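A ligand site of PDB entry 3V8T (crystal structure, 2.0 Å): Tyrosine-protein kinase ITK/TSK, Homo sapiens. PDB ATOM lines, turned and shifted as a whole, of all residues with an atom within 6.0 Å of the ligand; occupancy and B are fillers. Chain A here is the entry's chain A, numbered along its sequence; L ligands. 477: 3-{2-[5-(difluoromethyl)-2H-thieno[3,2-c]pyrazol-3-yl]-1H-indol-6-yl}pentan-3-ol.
The backbone NH of Met 84 lies close to a nitrogen (NAB) of the ligand. The backbone carbonyl oxygen (O) of Met 84 sits at hydrogen-bond distance from a nitrogen (NAE) of the ligand, at 2.8 Å. The backbone carbonyl oxygen (O) of Glu 82 lies close to a nitrogen (NAA) of the ligand (2.9 Å).
O of Ala 35 sits at hydrogen-bond distance from N of Phe 81 (2.9 Å). NZ of Lys 37 lies within salt-bridge range of OD2 of Asp 146 (3.0 Å). N of Ile 15 sits at hydrogen-bond distance from O of Val 23, 2.8 Å away. The backbone NH of Val 23 is in hydrogen-bond range of the backbone carbonyl oxygen of Gly 16.
OG of Ser 145 sits close to FAZ of the ligand (3.2 Å). Residues that only touch the ligand: Ile 15, Val 23, Ala 35, Lys 37, Phe 81, Phe 83, Glu 85, His 86, Gly 87, Leu 135 and Asp 146. Hydrophobic or aromatic side chains within 4 Å of the ligand: Ile 15, Val 23, Ala 35, Phe 81, Phe 83, Met 84 and Leu 135. Within 4 Å of the ligand: Ile 15, Val 23, Ala 35, Lys 37, Phe 81, Glu 82, Phe 83, Met 84, Glu 85, His 86, Gly 87, Leu 135, Ser 145 and Asp 146.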
ATOM      1  N   ILE A  15      -4.369  -5.876  -8.940  1.00  0.00           N
ATOM      2  CA  ILE A  15      -3.292  -6.809  -9.295  1.00  0.00           C
ATOM      3  C   ILE A  15      -3.789  -8.217  -9.660  1.00  0.00           C
ATOM      4  O   ILE A  15      -2.994  -9.045 -10.141  1.00  0.00           O
ATOM      5  CB  ILE A  15      -2.171  -6.816  -8.200  1.00  0.00           C
ATOM      6  CG1 ILE A  15      -2.737  -7.224  -6.813  1.00  0.00           C
ATOM      7  CG2 ILE A  15      -1.451  -5.448  -8.170  1.00  0.00           C
ATOM      8  CD1 ILE A  15      -1.716  -7.406  -5.661  1.00  0.00           C
ATOM      9  N   GLY A  16      -5.067  -8.483  -9.432  1.00  0.00           N
ATOM     10  CA  GLY A  16      -5.703  -9.763  -9.723  1.00  0.00           C
ATOM     11  C   GLY A  16      -7.206  -9.679  -9.827  1.00  0.00           C
ATOM     12  O   GLY A  16      -7.826  -8.780  -9.246  1.00  0.00           O
ATOM     13  N   VAL A  23      -8.359  -8.608  -6.530  1.00  0.00           N
ATOM     14  CA  VAL A  23      -7.231  -8.471  -5.608  1.00  0.00           C
ATOM     15  C   VAL A  23      -6.556  -7.129  -5.888  1.00  0.00           C
ATOM     16  O   VAL A  23      -6.193  -6.839  -7.034  1.00  0.00           O
ATOM     17  CB  VAL A  23      -6.238  -9.664  -5.654  1.00  0.00           C
ATOM     18  CG1 VAL A  23      -5.042  -9.451  -4.722  1.00  0.00           C
ATOM     19  CG2 VAL A  23      -6.937 -10.985  -5.318  1.00  0.00           C
ATOM     20  N   LEU A  25      -3.512  -4.215  -4.586  1.00  0.00           N
ATOM     21  CA  LEU A  25      -2.332  -3.882  -3.816  1.00  0.00           C
ATOM     22  C   LEU A  25      -2.760  -2.631  -3.048  1.00  0.00           C
ATOM     23  O   LEU A  25      -3.383  -1.737  -3.621  1.00  0.00           O
ATOM     24  CB  LEU A  25      -1.120  -3.573  -4.724  1.00  0.00           C
ATOM     25  CG  LEU A  25       0.057  -2.788  -4.106  1.00  0.00           C
ATOM     26  CD1 LEU A  25       0.781  -3.601  -3.034  1.00  0.00           C
ATOM     27  CD2 LEU A  25       1.033  -2.350  -5.157  1.00  0.00           C
ATOM     28  N   ALA A  35      -2.635  -7.033   0.490  1.00  0.00           N
ATOM     29  CA  ALA A  35      -3.358  -7.522  -0.672  1.00  0.00           C
ATOM     30  C   ALA A  35      -4.811  -7.581  -0.227  1.00  0.00           C
ATOM     31  O   ALA A  35      -5.159  -8.370   0.650  1.00  0.00           O
ATOM     32  CB  ALA A  35      -2.861  -8.901  -1.082  1.00  0.00           C
ATOM     33  N   LYS A  37      -8.570  -8.354  -0.892  1.00  0.00           N
ATOM     34  CA  LYS A  37      -9.425  -9.205  -1.713  1.00  0.00           C
ATOM     35  C   LYS A  37     -10.889  -8.803  -1.566  1.00  0.00           C
ATOM     36  O   LYS A  37     -11.516  -9.130  -0.561  1.00  0.00           O
ATOM     37  CB  LYS A  37      -9.211 -10.693  -1.348  1.00  0.00           C
ATOM     38  CG  LYS A  37      -9.858 -11.669  -2.335  1.00  0.00           C
ATOM     39  CD  LYS A  37      -9.748 -13.101  -1.852  1.00  0.00           C
ATOM     40  CE  LYS A  37     -10.421 -14.060  -2.799  1.00  0.00           C
ATOM     41  NZ  LYS A  37     -10.363 -15.459  -2.301  1.00  0.00           N
ATOM     42  N   MET A  56      -8.959 -19.141   8.712  1.00  0.00           N
ATOM     43  CA  MET A  56      -7.566 -18.840   8.363  1.00  0.00           C
ATOM     44  C   MET A  56      -6.809 -18.082   9.458  1.00  0.00           C
ATOM     45  O   MET A  56      -5.624 -18.328   9.656  1.00  0.00           O
ATOM     46  CB  MET A  56      -7.461 -18.088   7.028  1.00  0.00           C
ATOM     47  CG  MET A  56      -7.817 -18.931   5.813  1.00  0.00           C
ATOM     48  SD  MET A  56      -7.372 -18.157   4.234  1.00  0.00           S
ATOM     49  CE  MET A  56      -8.654 -16.915   4.109  1.00  0.00           C
ATOM     50  N   VAL A  65      -0.718 -18.531   4.198  1.00  0.00           N
ATOM     51  CA  VAL A  65      -0.937 -17.080   4.125  1.00  0.00           C
ATOM     52  C   VAL A  65      -1.645 -16.528   5.382  1.00  0.00           C
ATOM     53  O   VAL A  65      -2.464 -17.225   5.991  1.00  0.00           O
ATOM     54  CB  VAL A  65      -1.593 -16.635   2.781  1.00  0.00           C
ATOM     55  CG1 VAL A  65      -3.082 -16.948   2.738  1.00  0.00           C
ATOM     56  CG2 VAL A  65      -1.315 -15.162   2.487  1.00  0.00           C
ATOM     57  N   PHE A  81      -5.195  -9.275   3.451  1.00  0.00           N
ATOM     58  CA  PHE A  81      -4.107 -10.247   3.545  1.00  0.00           C
ATOM     59  C   PHE A  81      -2.749  -9.574   3.583  1.00  0.00           C
ATOM     60  O   PHE A  81      -2.604  -8.434   3.114  1.00  0.00           O
ATOM     61  CB  PHE A  81      -4.125 -11.173   2.311  1.00  0.00           C
ATOM     62  CG  PHE A  81      -5.260 -12.154   2.214  1.00  0.00           C
ATOM     63  CD1 PHE A  81      -6.431 -11.837   1.544  1.00  0.00           C
ATOM     64  CD2 PHE A  81      -5.138 -13.445   2.729  1.00  0.00           C
ATOM     65  CE1 PHE A  81      -7.466 -12.756   1.411  1.00  0.00           C
ATOM     66  CE2 PHE A  81      -6.174 -14.371   2.609  1.00  0.00           C
ATOM     67  CZ  PHE A  81      -7.340 -14.019   1.958  1.00  0.00           C
ATOM     68  N   GLU A  82      -1.728 -10.303   4.060  1.00  0.00           N
ATOM     69  CA  GLU A  82      -0.338  -9.859   4.007  1.00  0.00           C
ATOM     70  C   GLU A  82       0.018  -9.840   2.508  1.00  0.00           C
ATOM     71  O   GLU A  82      -0.525 -10.652   1.745  1.00  0.00           O
ATOM     72  CB  GLU A  82       0.588 -10.816   4.776  1.00  0.00           C
ATOM     73  CG  GLU A  82       0.620 -12.245   4.241  1.00  0.00           C
ATOM     74  CD  GLU A  82       1.654 -13.169   4.849  1.00  0.00           C
ATOM     75  OE1 GLU A  82       2.781 -12.719   5.120  1.00  0.00           O
ATOM     76  OE2 GLU A  82       1.337 -14.374   5.008  1.00  0.00           O
ATOM     77  N   PHE A  83       0.877  -8.916   2.087  1.00  0.00           N
ATOM     78  CA  PHE A  83       1.257  -8.837   0.684  1.00  0.00           C
ATOM     79  C   PHE A  83       2.387  -9.804   0.361  1.00  0.00           C
ATOM     80  O   PHE A  83       3.425  -9.775   1.034  1.00  0.00           O
ATOM     81  CB  PHE A  83       1.607  -7.394   0.274  1.00  0.00           C
ATOM     82  CG  PHE A  83       1.987  -7.251  -1.185  1.00  0.00           C
ATOM     83  CD1 PHE A  83       1.021  -7.328  -2.180  1.00  0.00           C
ATOM     84  CD2 PHE A  83       3.311  -7.044  -1.552  1.00  0.00           C
ATOM     85  CE1 PHE A  83       1.379  -7.204  -3.530  1.00  0.00           C
ATOM     86  CE2 PHE A  83       3.662  -6.923  -2.896  1.00  0.00           C
ATOM     87  CZ  PHE A  83       2.696  -7.006  -3.879  1.00  0.00           C
ATOM     88  N   MET A  84       2.185 -10.649  -0.650  1.00  0.00           N
ATOM     89  CA  MET A  84       3.192 -11.603  -1.121  1.00  0.00           C
ATOM     90  C   MET A  84       3.789 -11.029  -2.399  1.00  0.00           C
ATOM     91  O   MET A  84       3.093 -10.891  -3.400  1.00  0.00           O
ATOM     92  CB  MET A  84       2.591 -13.011  -1.325  1.00  0.00           C
ATOM     93  CG  MET A  84       2.067 -13.638  -0.032  1.00  0.00           C
ATOM     94  SD  MET A  84       3.354 -14.081   1.158  1.00  0.00           S
ATOM     95  CE  MET A  84       3.887 -15.632   0.480  1.00  0.00           C
ATOM     96  N   GLU A  85       5.076 -10.627  -2.319  1.00  0.00           N
ATOM     97  CA  GLU A  85       5.840  -9.954  -3.372  1.00  0.00           C
ATOM     98  C   GLU A  85       5.788 -10.508  -4.792  1.00  0.00           C
ATOM     99  O   GLU A  85       5.798  -9.725  -5.743  1.00  0.00           O
ATOM    100  CB  GLU A  85       7.294  -9.701  -2.940  1.00  0.00           C
ATOM    101  CG  GLU A  85       7.457  -8.618  -1.874  1.00  0.00           C
ATOM    102  CD  GLU A  85       7.356  -7.179  -2.329  1.00  0.00           C
ATOM    103  OE1 GLU A  85       7.912  -6.844  -3.396  1.00  0.00           O
ATOM    104  OE2 GLU A  85       6.778  -6.371  -1.562  1.00  0.00           O
ATOM    105  N   HIS A  86       5.753 -11.849  -4.952  1.00  0.00           N
ATOM    106  CA  HIS A  86       5.769 -12.442  -6.292  1.00  0.00           C
ATOM    107  C   HIS A  86       4.455 -13.026  -6.823  1.00  0.00           C
ATOM    108  O   HIS A  86       4.458 -13.715  -7.841  1.00  0.00           O
ATOM    109  CB  HIS A  86       6.953 -13.404  -6.443  1.00  0.00           C
ATOM    110  CG  HIS A  86       8.288 -12.770  -6.212  1.00  0.00           C
ATOM    111  ND1 HIS A  86       8.852 -11.904  -7.144  1.00  0.00           N
ATOM    112  CD2 HIS A  86       9.143 -12.896  -5.166  1.00  0.00           C
ATOM    113  CE1 HIS A  86      10.010 -11.527  -6.630  1.00  0.00           C
ATOM    114  NE2 HIS A  86      10.224 -12.100  -5.443  1.00  0.00           N
ATOM    115  N   GLY A  87       3.342 -12.698  -6.166  1.00  0.00           N
ATOM    116  CA  GLY A  87       2.008 -13.129  -6.572  1.00  0.00           C
ATOM    117  C   GLY A  87       1.759 -14.615  -6.546  1.00  0.00           C
ATOM    118  O   GLY A  87       2.455 -15.352  -5.833  1.00  0.00           O
ATOM    119  N   CYS A  88       0.749 -15.070  -7.323  1.00  0.00           N
ATOM    120  CA  CYS A  88       0.406 -16.494  -7.348  1.00  0.00           C
ATOM    121  C   CYS A  88       1.451 -17.344  -8.051  1.00  0.00           C
ATOM    122  O   CYS A  88       2.080 -16.897  -9.026  1.00  0.00           O
ATOM    123  CB  CYS A  88      -1.013 -16.743  -7.864  1.00  0.00           C
ATOM    124  SG  CYS A  88      -1.215 -16.469  -9.639  1.00  0.00           S
ATOM    125  N   TYR A  92       3.957 -16.979 -11.493  1.00  0.00           N
ATOM    126  CA  TYR A  92       5.395 -16.883 -11.213  1.00  0.00           C
ATOM    127  C   TYR A  92       6.224 -17.957 -11.929  1.00  0.00           C
ATOM    128  O   TYR A  92       7.315 -17.661 -12.405  1.00  0.00           O
ATOM    129  CB  TYR A  92       5.667 -16.896  -9.699  1.00  0.00           C
ATOM    130  CG  TYR A  92       7.115 -16.631  -9.333  1.00  0.00           C
ATOM    131  CD1 TYR A  92       7.649 -15.356  -9.422  1.00  0.00           C
ATOM    132  CD2 TYR A  92       7.933 -17.656  -8.865  1.00  0.00           C
ATOM    133  CE1 TYR A  92       8.980 -15.103  -9.067  1.00  0.00           C
ATOM    134  CE2 TYR A  92       9.263 -17.418  -8.502  1.00  0.00           C
ATOM    135  CZ  TYR A  92       9.777 -16.131  -8.610  1.00  0.00           C
ATOM    136  OH  TYR A  92      11.085 -15.887  -8.252  1.00  0.00           O
ATOM    137  N   LEU A 135       0.936 -18.783  -3.050  1.00  0.00           N
ATOM    138  CA  LEU A 135       1.572 -17.476  -3.230  1.00  0.00           C
ATOM    139  C   LEU A 135       3.082 -17.524  -3.043  1.00  0.00           C
ATOM    140  O   LEU A 135       3.581 -18.364  -2.297  1.00  0.00           O
ATOM    141  CB  LEU A 135       0.942 -16.437  -2.301  1.00  0.00           C
ATOM    142  CG  LEU A 135      -0.545 -16.158  -2.503  1.00  0.00           C
ATOM    143  CD1 LEU A 135      -1.151 -15.595  -1.251  1.00  0.00           C
ATOM    144  CD2 LEU A 135      -0.785 -15.225  -3.698  1.00  0.00           C
ATOM    145  N   SER A 145      -2.701 -20.595   0.010  1.00  0.00           N
ATOM    146  CA  SER A 145      -3.742 -19.583   0.200  1.00  0.00           C
ATOM    147  C   SER A 145      -5.144 -20.192   0.027  1.00  0.00           C
ATOM    148  O   SER A 145      -5.251 -21.325  -0.452  1.00  0.00           O
ATOM    149  CB  SER A 145      -3.548 -18.425  -0.781  1.00  0.00           C
ATOM    150  OG  SER A 145      -4.422 -17.344  -0.485  1.00  0.00           O
ATOM    151  N   ASP A 146      -6.194 -19.444   0.424  1.00  0.00           N
ATOM    152  CA  ASP A 146      -7.622 -19.830   0.330  1.00  0.00           C
ATOM    153  C   ASP A 146      -7.900 -21.232   0.883  1.00  0.00           C
ATOM    154  O   ASP A 146      -8.529 -22.069   0.215  1.00  0.00           O
ATOM    155  CB  ASP A 146      -8.143 -19.649  -1.110  1.00  0.00           C
ATOM    156  CG  ASP A 146      -7.878 -18.275  -1.717  1.00  0.00           C
ATOM    157  OD1 ASP A 146      -7.302 -18.214  -2.827  1.00  0.00           O
ATOM    158  OD2 ASP A 146      -8.253 -17.257  -1.081  1.00  0.00           O
HETATM  159  CAU 477 L   1       2.003  -6.343  -7.947  1.00  0.00           C
HETATM  160  CAT 477 L   1       3.142  -7.357  -7.920  1.00  0.00           C
HETATM  161  CAR 477 L   1       2.748  -8.687  -8.575  1.00  0.00           C
HETATM  162  CAW 477 L   1       3.970  -9.607  -8.575  1.00  0.00           C
HETATM  163  CAX 477 L   1       3.746 -10.865  -9.416  1.00  0.00           C
HETATM  164  OAS 477 L   1       2.345  -8.439  -9.936  1.00  0.00           O
HETATM  165  CAJ 477 L   1       1.602  -9.354  -7.782  1.00  0.00           C
HETATM  166  CAI 477 L   1       1.722  -9.534  -6.408  1.00  0.00           C
HETATM  167  CAK 477 L   1       0.432  -9.798  -8.426  1.00  0.00           C
HETATM  168  CAL 477 L   1      -0.594 -10.405  -7.693  1.00  0.00           C
HETATM  169  CAG 477 L   1      -0.460 -10.588  -6.319  1.00  0.00           C
HETATM  170  CAF 477 L   1      -1.249 -11.108  -5.380  1.00  0.00           C
HETATM  171  CAH 477 L   1       0.683 -10.131  -5.670  1.00  0.00           C
HETATM  172  NAE 477 L   1       0.550 -10.431  -4.391  1.00  0.00           N
HETATM  173  CAD 477 L   1      -0.628 -11.022  -4.197  1.00  0.00           C
HETATM  174  CAC 477 L   1      -1.092 -11.451  -2.951  1.00  0.00           C
HETATM  175  NAB 477 L   1      -0.512 -11.297  -1.759  1.00  0.00           N
HETATM  176  NAA 477 L   1      -1.208 -11.806  -0.866  1.00  0.00           N
HETATM  177  CAM 477 L   1      -2.342 -12.331  -1.343  1.00  0.00           C
HETATM  178  CAQ 477 L   1      -3.464 -12.967  -0.946  1.00  0.00           C
HETATM  179  CAN 477 L   1      -2.293 -12.111  -2.729  1.00  0.00           C
HETATM  180  SAO 477 L   1      -3.691 -12.772  -3.398  1.00  0.00           S
HETATM  181  CAP 477 L   1      -4.306 -13.300  -1.940  1.00  0.00           C
HETATM  182  CAV 477 L   1      -5.634 -14.051  -1.770  1.00  0.00           C
HETATM  183  FAZ 477 L   1      -5.795 -14.412  -0.452  1.00  0.00           F
HETATM  184  FAY 477 L   1      -6.687 -13.250  -2.179  1.00  0.00           F
